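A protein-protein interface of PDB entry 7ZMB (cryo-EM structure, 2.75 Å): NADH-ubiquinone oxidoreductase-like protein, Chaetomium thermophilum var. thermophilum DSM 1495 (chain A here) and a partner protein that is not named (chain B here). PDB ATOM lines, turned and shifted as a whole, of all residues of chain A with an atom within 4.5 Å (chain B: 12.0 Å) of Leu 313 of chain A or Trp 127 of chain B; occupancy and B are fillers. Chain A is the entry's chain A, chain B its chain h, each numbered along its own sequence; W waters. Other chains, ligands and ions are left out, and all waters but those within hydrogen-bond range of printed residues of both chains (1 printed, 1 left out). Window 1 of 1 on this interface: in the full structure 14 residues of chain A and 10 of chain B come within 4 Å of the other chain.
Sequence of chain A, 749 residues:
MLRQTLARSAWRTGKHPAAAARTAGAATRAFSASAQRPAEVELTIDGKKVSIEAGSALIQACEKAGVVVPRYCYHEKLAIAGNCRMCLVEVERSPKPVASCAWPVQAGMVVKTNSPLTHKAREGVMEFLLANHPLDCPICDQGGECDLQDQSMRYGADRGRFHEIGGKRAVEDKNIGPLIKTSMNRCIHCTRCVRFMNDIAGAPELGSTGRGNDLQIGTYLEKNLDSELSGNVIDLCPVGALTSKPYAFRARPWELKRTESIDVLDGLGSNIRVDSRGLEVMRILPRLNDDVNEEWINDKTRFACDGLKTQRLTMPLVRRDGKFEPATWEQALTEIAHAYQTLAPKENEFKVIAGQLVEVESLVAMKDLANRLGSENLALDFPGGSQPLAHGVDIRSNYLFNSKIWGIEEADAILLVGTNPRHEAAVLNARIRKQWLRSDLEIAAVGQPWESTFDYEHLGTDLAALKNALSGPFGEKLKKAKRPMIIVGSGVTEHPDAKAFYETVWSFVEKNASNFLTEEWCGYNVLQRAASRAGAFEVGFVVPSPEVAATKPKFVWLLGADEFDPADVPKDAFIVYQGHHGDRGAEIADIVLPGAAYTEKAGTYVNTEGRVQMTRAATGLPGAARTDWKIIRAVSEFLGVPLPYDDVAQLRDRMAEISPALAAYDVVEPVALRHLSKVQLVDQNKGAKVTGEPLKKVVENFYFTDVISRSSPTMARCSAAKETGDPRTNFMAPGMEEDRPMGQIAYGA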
ATOM      1  N   GLN A 311      -0.771  -5.133   0.821  1.00  0.00           N
ATOM      2  CA  GLN A 311      -1.296  -3.797   1.071  1.00  0.00           C
ATOM      3  C   GLN A 311      -1.123  -2.940  -0.164  1.00  0.00           C
ATOM      4  O   GLN A 311      -0.703  -1.784  -0.107  1.00  0.00           O
ATOM      5  CB  GLN A 311      -0.614  -3.149   2.269  1.00  0.00           C
ATOM      6  CG  GLN A 311      -0.803  -3.884   3.581  1.00  0.00           C
ATOM      7  CD  GLN A 311      -2.013  -3.395   4.333  1.00  0.00           C
ATOM      8  OE1 GLN A 311      -2.922  -2.813   3.750  1.00  0.00           O
ATOM      9  NE2 GLN A 311      -2.030  -3.622   5.641  1.00  0.00           N
ATOM     10  N   ARG A 312      -1.454  -3.516  -1.311  1.00  0.00           N
ATOM     11  CA  ARG A 312      -1.077  -2.914  -2.568  1.00  0.00           C
ATOM     12  C   ARG A 312      -2.046  -1.808  -2.959  1.00  0.00           C
ATOM     13  O   ARG A 312      -3.183  -1.735  -2.493  1.00  0.00           O
ATOM     14  CB  ARG A 312      -1.000  -3.973  -3.664  1.00  0.00           C
ATOM     15  CG  ARG A 312       0.002  -5.080  -3.381  1.00  0.00           C
ATOM     16  CD  ARG A 312       1.430  -4.572  -3.406  1.00  0.00           C
ATOM     17  NE  ARG A 312       1.698  -3.778  -4.595  1.00  0.00           N
ATOM     18  CZ  ARG A 312       2.137  -4.276  -5.742  1.00  0.00           C
ATOM     19  NH1 ARG A 312       2.360  -5.575  -5.862  1.00  0.00           N
ATOM     20  NH2 ARG A 312       2.351  -3.473  -6.770  1.00  0.00           N
ATOM     21  N   LEU A 313      -1.555  -0.926  -3.816  1.00  0.00           N
ATOM     22  CA  LEU A 313      -2.342   0.133  -4.419  1.00  0.00           C
ATOM     23  C   LEU A 313      -2.679  -0.306  -5.835  1.00  0.00           C
ATOM     24  O   LEU A 313      -1.778  -0.600  -6.625  1.00  0.00           O
ATOM     25  CB  LEU A 313      -1.562   1.448  -4.426  1.00  0.00           C
ATOM     26  CG  LEU A 313      -1.129   1.970  -3.057  1.00  0.00           C
ATOM     27  CD1 LEU A 313      -0.212   3.165  -3.190  1.00  0.00           C
ATOM     28  CD2 LEU A 313      -2.335   2.317  -2.223  1.00  0.00           C
ATOM     29  N   THR A 314      -3.968  -0.377  -6.145  1.00  0.00           N
ATOM     30  CA  THR A 314      -4.404  -0.809  -7.459  1.00  0.00           C
ATOM     31  C   THR A 314      -5.262   0.210  -8.183  1.00  0.00           C
ATOM     32  O   THR A 314      -5.543   0.017  -9.366  1.00  0.00           O
ATOM     33  CB  THR A 314      -5.182  -2.129  -7.369  1.00  0.00           C
ATOM     34  OG1 THR A 314      -6.202  -2.018  -6.372  1.00  0.00           O
ATOM     35  CG2 THR A 314      -4.255  -3.277  -7.021  1.00  0.00           C
ATOM     36  N   MET A 315      -5.687   1.277  -7.522  1.00  0.00           N
ATOM     37  CA  MET A 315      -6.578   2.241  -8.135  1.00  0.00           C
ATOM     38  C   MET A 315      -6.208   3.640  -7.678  1.00  0.00           C
ATOM     39  O   MET A 315      -5.698   3.820  -6.567  1.00  0.00           O
ATOM     40  CB  MET A 315      -8.030   1.938  -7.762  1.00  0.00           C
ATOM     41  CG  MET A 315      -8.193   1.618  -6.291  1.00  0.00           C
ATOM     42  SD  MET A 315      -9.914   1.591  -5.840  1.00  0.00           S
ATOM     43  CE  MET A 315     -10.501   0.654  -7.227  1.00  0.00           C
ATOM     44  N   LEU A 317      -6.828   7.064  -5.967  1.00  0.00           N
ATOM     45  CA  LEU A 317      -7.704   7.537  -4.908  1.00  0.00           C
ATOM     46  C   LEU A 317      -7.560   9.042  -4.775  1.00  0.00           C
ATOM     47  O   LEU A 317      -6.445   9.557  -4.667  1.00  0.00           O
ATOM     48  CB  LEU A 317      -7.388   6.867  -3.573  1.00  0.00           C
ATOM     49  CG  LEU A 317      -7.399   5.344  -3.563  1.00  0.00           C
ATOM     50  CD1 LEU A 317      -6.827   4.847  -2.262  1.00  0.00           C
ATOM     51  CD2 LEU A 317      -8.800   4.808  -3.791  1.00  0.00           C
ATOM     52  N   PHE A 324     -10.910   8.597   1.233  1.00  0.00           N
ATOM     53  CA  PHE A 324     -10.276   8.234  -0.025  1.00  0.00           C
ATOM     54  C   PHE A 324     -11.293   7.513  -0.896  1.00  0.00           C
ATOM     55  O   PHE A 324     -11.750   6.420  -0.547  1.00  0.00           O
ATOM     56  CB  PHE A 324      -9.049   7.354   0.203  1.00  0.00           C
ATOM     57  CG  PHE A 324      -7.781   8.119   0.354  1.00  0.00           C
ATOM     58  CD1 PHE A 324      -7.415   9.073  -0.577  1.00  0.00           C
ATOM     59  CD2 PHE A 324      -6.936   7.875   1.416  1.00  0.00           C
ATOM     60  CE1 PHE A 324      -6.238   9.778  -0.438  1.00  0.00           C
ATOM     61  CE2 PHE A 324      -5.765   8.579   1.560  1.00  0.00           C
ATOM     62  CZ  PHE A 324      -5.421   9.532   0.631  1.00  0.00           C
ATOM     63  N   TYR A 577       0.931  11.254  -3.798  1.00  0.00           N
ATOM     64  CA  TYR A 577       1.729  10.082  -3.473  1.00  0.00           C
ATOM     65  C   TYR A 577       1.670   9.081  -4.612  1.00  0.00           C
ATOM     66  O   TYR A 577       0.586   8.670  -5.030  1.00  0.00           O
ATOM     67  CB  TYR A 577       1.268   9.413  -2.181  1.00  0.00           C
ATOM     68  CG  TYR A 577       2.044   8.162  -1.906  1.00  0.00           C
ATOM     69  CD1 TYR A 577       3.297   8.223  -1.325  1.00  0.00           C
ATOM     70  CD2 TYR A 577       1.543   6.914  -2.261  1.00  0.00           C
ATOM     71  CE1 TYR A 577       4.020   7.089  -1.087  1.00  0.00           C
ATOM     72  CE2 TYR A 577       2.266   5.773  -2.030  1.00  0.00           C
ATOM     73  CZ  TYR A 577       3.504   5.867  -1.444  1.00  0.00           C
ATOM     74  OH  TYR A 577       4.229   4.732  -1.200  1.00  0.00           O
ATOM     75  N   GLY A 579       3.256   5.283  -5.663  1.00  0.00           N
ATOM     76  CA  GLY A 579       3.885   4.134  -5.054  1.00  0.00           C
ATOM     77  C   GLY A 579       3.029   2.900  -5.241  1.00  0.00           C
ATOM     78  O   GLY A 579       2.048   2.908  -5.981  1.00  0.00           O
ATOM     79  N   HIS A 580       3.433   1.835  -4.555  1.00  0.00           N
ATOM     80  CA  HIS A 580       2.780   0.546  -4.691  1.00  0.00           C
ATOM     81  C   HIS A 580       2.191   0.020  -3.393  1.00  0.00           C
ATOM     82  O   HIS A 580       1.484  -0.990  -3.422  1.00  0.00           O
ATOM     83  CB  HIS A 580       3.756  -0.493  -5.268  1.00  0.00           C
ATOM     84  CG  HIS A 580       5.122  -0.456  -4.657  1.00  0.00           C
ATOM     85  ND1 HIS A 580       5.372  -0.863  -3.365  1.00  0.00           N
ATOM     86  CD2 HIS A 580       6.316  -0.074  -5.166  1.00  0.00           C
ATOM     87  CE1 HIS A 580       6.658  -0.728  -3.103  1.00  0.00           C
ATOM     88  NE2 HIS A 580       7.254  -0.251  -4.179  1.00  0.00           N
ATOM     89  N   HIS A 581       2.433   0.678  -2.269  1.00  0.00           N
ATOM     90  CA  HIS A 581       1.918   0.227  -0.990  1.00  0.00           C
ATOM     91  C   HIS A 581       1.172   1.349  -0.299  1.00  0.00           C
ATOM     92  O   HIS A 581       1.556   2.515  -0.399  1.00  0.00           O
ATOM     93  CB  HIS A 581       3.034  -0.267  -0.085  1.00  0.00           C
ATOM     94  CG  HIS A 581       3.290  -1.729  -0.210  1.00  0.00           C
ATOM     95  ND1 HIS A 581       4.033  -2.264  -1.237  1.00  0.00           N
ATOM     96  CD2 HIS A 581       2.883  -2.773   0.543  1.00  0.00           C
ATOM     97  CE1 HIS A 581       4.081  -3.573  -1.107  1.00  0.00           C
ATOM     98  NE2 HIS A 581       3.392  -3.909  -0.033  1.00  0.00           N
ATOM     99  N   GLY A 582       0.109   0.988   0.405  1.00  0.00           N
ATOM    100  CA  GLY A 582      -0.559   1.926   1.276  1.00  0.00           C
ATOM    101  C   GLY A 582       0.115   1.984   2.626  1.00  0.00           C
ATOM    102  O   GLY A 582      -0.049   1.080   3.446  1.00  0.00           O
ATOM    103  N   ALA A 586       1.122   7.217   1.581  1.00  0.00           N
ATOM    104  CA  ALA A 586      -0.160   7.250   0.889  1.00  0.00           C
ATOM    105  C   ALA A 586      -1.260   7.826   1.764  1.00  0.00           C
ATOM    106  O   ALA A 586      -2.189   8.464   1.258  1.00  0.00           O
ATOM    107  CB  ALA A 586      -0.543   5.846   0.427  1.00  0.00           C
ATOM    108  N   GLU A 587      -1.165   7.624   3.068  1.00  0.00           N
ATOM    109  CA  GLU A 587      -2.253   7.944   3.974  1.00  0.00           C
ATOM    110  C   GLU A 587      -2.306   9.415   4.362  1.00  0.00           C
ATOM    111  O   GLU A 587      -3.273   9.824   5.013  1.00  0.00           O
ATOM    112  CB  GLU A 587      -2.136   7.038   5.204  1.00  0.00           C
ATOM    113  CG  GLU A 587      -0.898   7.280   6.032  1.00  0.00           C
ATOM    114  CD  GLU A 587      -0.778   6.324   7.193  1.00  0.00           C
ATOM    115  OE1 GLU A 587      -1.660   5.452   7.336  1.00  0.00           O
ATOM    116  OE2 GLU A 587       0.206   6.434   7.954  1.00  0.00           O
ATOM    117  N   PRO A 594      -1.386   4.510  -8.248  1.00  0.00           N
ATOM    118  CA  PRO A 594      -0.769   3.185  -8.114  1.00  0.00           C
ATOM    119  C   PRO A 594       0.304   2.938  -9.164  1.00  0.00           C
ATOM    120  O   PRO A 594       0.037   2.931 -10.364  1.00  0.00           O
ATOM    121  CB  PRO A 594      -1.959   2.237  -8.289  1.00  0.00           C
ATOM    122  CG  PRO A 594      -2.908   3.006  -9.125  1.00  0.00           C
ATOM    123  CD  PRO A 594      -2.798   4.414  -8.646  1.00  0.00           C
ATOM    124  N   ALA A 625      -2.787  -0.453 -11.793  1.00  0.00           N
ATOM    125  CA  ALA A 625      -1.514   0.214 -11.603  1.00  0.00           C
ATOM    126  C   ALA A 625      -0.816   0.431 -12.937  1.00  0.00           C
ATOM    127  O   ALA A 625      -1.032  -0.295 -13.908  1.00  0.00           O
ATOM    128  CB  ALA A 625      -0.619  -0.593 -10.673  1.00  0.00           C
ATOM    129  N   PRO B 122      -8.590 -14.895  -2.962  1.00  0.00           N
ATOM    130  CA  PRO B 122      -7.877 -14.124  -3.984  1.00  0.00           C
ATOM    131  C   PRO B 122      -6.398 -13.988  -3.656  1.00  0.00           C
ATOM    132  O   PRO B 122      -5.975 -14.134  -2.507  1.00  0.00           O
ATOM    133  CB  PRO B 122      -8.589 -12.766  -3.964  1.00  0.00           C
ATOM    134  CG  PRO B 122      -9.266 -12.712  -2.655  1.00  0.00           C
ATOM    135  CD  PRO B 122      -9.692 -14.115  -2.383  1.00  0.00           C
ATOM    136  N   LYS B 123      -5.609 -13.708  -4.689  1.00  0.00           N
ATOM    137  CA  LYS B 123      -4.164 -13.853  -4.564  1.00  0.00           C
ATOM    138  C   LYS B 123      -3.491 -12.550  -4.152  1.00  0.00           C
ATOM    139  O   LYS B 123      -2.394 -12.568  -3.586  1.00  0.00           O
ATOM    140  CB  LYS B 123      -3.587 -14.383  -5.874  1.00  0.00           C
ATOM    141  CG  LYS B 123      -4.222 -15.695  -6.292  1.00  0.00           C
ATOM    142  CD  LYS B 123      -3.221 -16.660  -6.862  1.00  0.00           C
ATOM    143  CE  LYS B 123      -3.921 -17.769  -7.625  1.00  0.00           C
ATOM    144  NZ  LYS B 123      -4.861 -18.530  -6.762  1.00  0.00           N
ATOM    145  N   ILE B 124      -4.129 -11.415  -4.403  1.00  0.00           N
ATOM    146  CA  ILE B 124      -3.575 -10.114  -4.054  1.00  0.00           C
ATOM    147  C   ILE B 124      -4.634  -9.321  -3.298  1.00  0.00           C
ATOM    148  O   ILE B 124      -5.796  -9.272  -3.710  1.00  0.00           O
ATOM    149  CB  ILE B 124      -3.072  -9.367  -5.306  1.00  0.00           C
ATOM    150  CG1 ILE B 124      -2.274  -8.130  -4.912  1.00  0.00           C
ATOM    151  CG2 ILE B 124      -4.212  -9.019  -6.246  1.00  0.00           C
ATOM    152  CD1 ILE B 124      -1.495  -7.541  -6.044  1.00  0.00           C
ATOM    153  N   GLN B 125      -4.239  -8.731  -2.179  1.00  0.00           N
ATOM    154  CA  GLN B 125      -5.140  -7.960  -1.333  1.00  0.00           C
ATOM    155  C   GLN B 125      -4.811  -6.482  -1.453  1.00  0.00           C
ATOM    156  O   GLN B 125      -3.665  -6.077  -1.246  1.00  0.00           O
ATOM    157  CB  GLN B 125      -5.031  -8.398   0.125  1.00  0.00           C
ATOM    158  CG  GLN B 125      -5.324  -9.865   0.361  1.00  0.00           C
ATOM    159  CD  GLN B 125      -6.809 -10.161   0.417  1.00  0.00           C
ATOM    160  OE1 GLN B 125      -7.536  -9.936  -0.550  1.00  0.00           O
ATOM    161  NE2 GLN B 125      -7.267 -10.667   1.555  1.00  0.00           N
ATOM    162  N   SER B 126      -5.816  -5.682  -1.776  1.00  0.00           N
ATOM    163  CA  SER B 126      -5.612  -4.256  -1.943  1.00  0.00           C
ATOM    164  C   SER B 126      -5.635  -3.544  -0.598  1.00  0.00           C
ATOM    165  O   SER B 126      -6.197  -4.028   0.390  1.00  0.00           O
ATOM    166  CB  SER B 126      -6.675  -3.663  -2.861  1.00  0.00           C
ATOM    167  OG  SER B 126      -7.958  -3.739  -2.269  1.00  0.00           O
ATOM    168  N   TRP B 127      -4.998  -2.381  -0.571  1.00  0.00           N
ATOM    169  CA  TRP B 127      -5.008  -1.525   0.606  1.00  0.00           C
ATOM    170  C   TRP B 127      -6.423  -1.061   0.923  1.00  0.00           C
ATOM    171  O   TRP B 127      -7.160  -0.639   0.033  1.00  0.00           O
ATOM    172  CB  TRP B 127      -4.106  -0.323   0.352  1.00  0.00           C
ATOM    173  CG  TRP B 127      -3.899   0.600   1.491  1.00  0.00           C
ATOM    174  CD1 TRP B 127      -3.513   0.277   2.751  1.00  0.00           C
ATOM    175  CD2 TRP B 127      -4.029   2.022   1.462  1.00  0.00           C
ATOM    176  NE1 TRP B 127      -3.404   1.407   3.515  1.00  0.00           N
ATOM    177  CE2 TRP B 127      -3.715   2.494   2.746  1.00  0.00           C
ATOM    178  CE3 TRP B 127      -4.387   2.944   0.474  1.00  0.00           C
ATOM    179  CZ2 TRP B 127      -3.748   3.846   3.071  1.00  0.00           C
ATOM    180  CZ3 TRP B 127      -4.420   4.280   0.795  1.00  0.00           C
ATOM    181  CH2 TRP B 127      -4.104   4.721   2.084  1.00  0.00           C
ATOM    182  N   GLU B 128      -6.805  -1.160   2.190  1.00  0.00           N
ATOM    183  CA  GLU B 128      -7.986  -0.439   2.635  1.00  0.00           C
ATOM    184  C   GLU B 128      -7.554   0.986   2.933  1.00  0.00           C
ATOM    185  O   GLU B 128      -6.786   1.218   3.873  1.00  0.00           O
ATOM    186  CB  GLU B 128      -8.618  -1.076   3.869  1.00  0.00           C
ATOM    187  CG  GLU B 128      -9.466  -2.293   3.567  1.00  0.00           C
ATOM    188  CD  GLU B 128     -10.675  -1.955   2.720  1.00  0.00           C
ATOM    189  OE1 GLU B 128     -11.249  -0.862   2.910  1.00  0.00           O
ATOM    190  OE2 GLU B 128     -11.048  -2.779   1.861  1.00  0.00           O
ATOM    191  N   PRO B 129      -8.005   1.953   2.143  1.00  0.00           N
ATOM    192  CA  PRO B 129      -7.543   3.329   2.323  1.00  0.00           C
ATOM    193  C   PRO B 129      -7.868   3.861   3.709  1.00  0.00           C
ATOM    194  O   PRO B 129      -8.949   3.630   4.249  1.00  0.00           O
ATOM    195  CB  PRO B 129      -8.301   4.096   1.238  1.00  0.00           C
ATOM    196  CG  PRO B 129      -8.660   3.081   0.236  1.00  0.00           C
ATOM    197  CD  PRO B 129      -8.860   1.804   0.959  1.00  0.00           C
ATOM    198  N   LYS B 130      -6.910   4.583   4.281  1.00  0.00           N
ATOM    199  CA  LYS B 130      -7.063   5.230   5.579  1.00  0.00           C
ATOM    200  C   LYS B 130      -6.521   6.652   5.436  1.00  0.00           C
ATOM    201  O   LYS B 130      -5.337   6.903   5.660  1.00  0.00           O
ATOM    202  CB  LYS B 130      -6.346   4.453   6.664  1.00  0.00           C
ATOM    203  CG  LYS B 130      -6.573   4.999   8.058  1.00  0.00           C
ATOM    204  CD  LYS B 130      -5.777   4.217   9.086  1.00  0.00           C
ATOM    205  CE  LYS B 130      -6.391   2.849   9.328  1.00  0.00           C
ATOM    206  NZ  LYS B 130      -5.691   2.114  10.418  1.00  0.00           N
ATOM    207  N   ALA B 131      -7.396   7.575   5.061  1.00  0.00           N
ATOM    208  CA  ALA B 131      -7.023   8.971   4.862  1.00  0.00           C
ATOM    209  C   ALA B 131      -6.822   9.622   6.220  1.00  0.00           C
ATOM    210  O   ALA B 131      -7.783  10.025   6.879  1.00  0.00           O
ATOM    211  CB  ALA B 131      -8.091   9.698   4.054  1.00  0.00           C
ATOM    212  N   ALA B 132      -5.568   9.726   6.645  1.00  0.00           N
ATOM    213  CA  ALA B 132      -5.265  10.349   7.922  1.00  0.00           C
ATOM    214  C   ALA B 132      -5.692  11.815   7.902  1.00  0.00           C
ATOM    215  O   ALA B 132      -5.634  12.471   6.857  1.00  0.00           O
ATOM    216  CB  ALA B 132      -3.774  10.238   8.233  1.00  0.00           C
ATOM    217  N   PRO B 133      -6.145  12.347   9.037  1.00  0.00           N
ATOM    218  CA  PRO B 133      -6.582  13.747   9.069  1.00  0.00           C
ATOM    219  C   PRO B 133      -5.445  14.691   8.715  1.00  0.00           C
ATOM    220  O   PRO B 133      -4.286  14.462   9.068  1.00  0.00           O
ATOM    221  CB  PRO B 133      -7.048  13.941  10.516  1.00  0.00           C
ATOM    222  CG  PRO B 133      -6.350  12.873  11.287  1.00  0.00           C
ATOM    223  CD  PRO B 133      -6.252  11.706  10.356  1.00  0.00           C
HETATM  224  O   HOH W   1     -10.003   6.619   3.455  1.00  0.00           O
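The backbone carbonyl oxygen of Gln 125 of chain B is in hydrogen-bond range of the backbone NH of Arg 312 of chain A (3.4 Å). The backbone carbonyl oxygen of Arg 312 of chain A is in hydrogen-bond range of the backbone NH of Trp 127 of chain B, 2.7 Å away. NE1 of Trp 127 of chain B is in hydrogen-bond range of O of Gly 582 of chain A, at 3.4 Å. O of Glu 587 of chain A sits at hydrogen-bond distance from N of Ala 132 of chain B (2.8 Å).
Leu 313 of chain A touches just one residue of chain B: Trp 127 (3.4 Å). Met 315 of chain A touches none of the printed residues of chain B. Phe 324 of chain A touches just these residues of chain B: Pro 129 and Ala 131. No residue of chain B comes within 4 Å of Gly 579 of chain A. No residue of chain B comes within 4 Å of His 581 of chain A. No residue of chain B comes within 4 Å of Ala 625 of chain A. Printed residues of chain A within 4 Å of Ile 124 of chain B: Arg 312. Of chain A, only Gln 311 (3.3 Å), Arg 312 (2.7 Å), Leu 313 (3.4 Å), Leu 317 (3.9 Å) and Gly 582 (3.4 Å) come within 4 Å of Trp 127 of chain B. Of the printed residues of chain A, Pro 129 of chain B touches Leu 317 (3.6 Å) and Phe 324 (3.5 Å). Pro 133 of chain B touches none of the printed residues of chain A. The nearest residue of chain A that does not touch Trp 127 of chain B is Ala 586 of chain A (4.1 Å).
The backbone carbonyl oxygen (O) of Gln 311 of chain A is in hydrogen-bond range of the backbone NH (N) of Gly 582 of chain A (2.9 Å). O of His 580 of chain A sits at hydrogen-bond distance from NE of Arg 312 of chain A (3.0 Å). N of Leu 313 of chain A sits at hydrogen-bond distance from O of His 580 of chain A (3.1 Å).
Of the 16 printed residues of chain A, 8 touch a printed residue of chain B. Hydrophobic or aromatic side chains of chain B within 4 Å of the printed part of chain A: Ile 124, Trp 127, Pro 129, Ala 131 and Ala 132.
Among the printed residues, pairs that only touch across the chains: Glu 587 of chain A with Lys 130 of chain B (3.2 Å), Gln 311 of chain A with Trp 127 of chain B (3.3 Å), Phe 324 of chain A with Ala 131 of chain B (3.4 Å), Leu 313 of chain A with Trp 127 of chain B (3.4 Å), Phe 324 of chain A with Pro 129 of chain B (3.5 Å), Arg 312 of chain A with Ser 126 of chain B (3.5 Å), Leu 317 of chain A with Pro 129 of chain B (3.6 Å), Gln 311 of chain A with Gln 125 of chain B (3.7 Å), Glu 587 of chain A with Ala 131 of chain B (3.8 Å), Thr 314 of chain A with Ser 126 of chain B (3.9 Å), Arg 312 of chain A with Ile 124 of chain B (3.9 Å) and Leu 317 of chain A with Trp 127 of chain B (3.9 Å).
Water W1 lies within hydrogen-bond range of N of Phe 324 of chain A (3.1 Å), N of Ala 131 of chain B (3.2 Å) and O of Pro 129 of chain B (3.3 Å).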
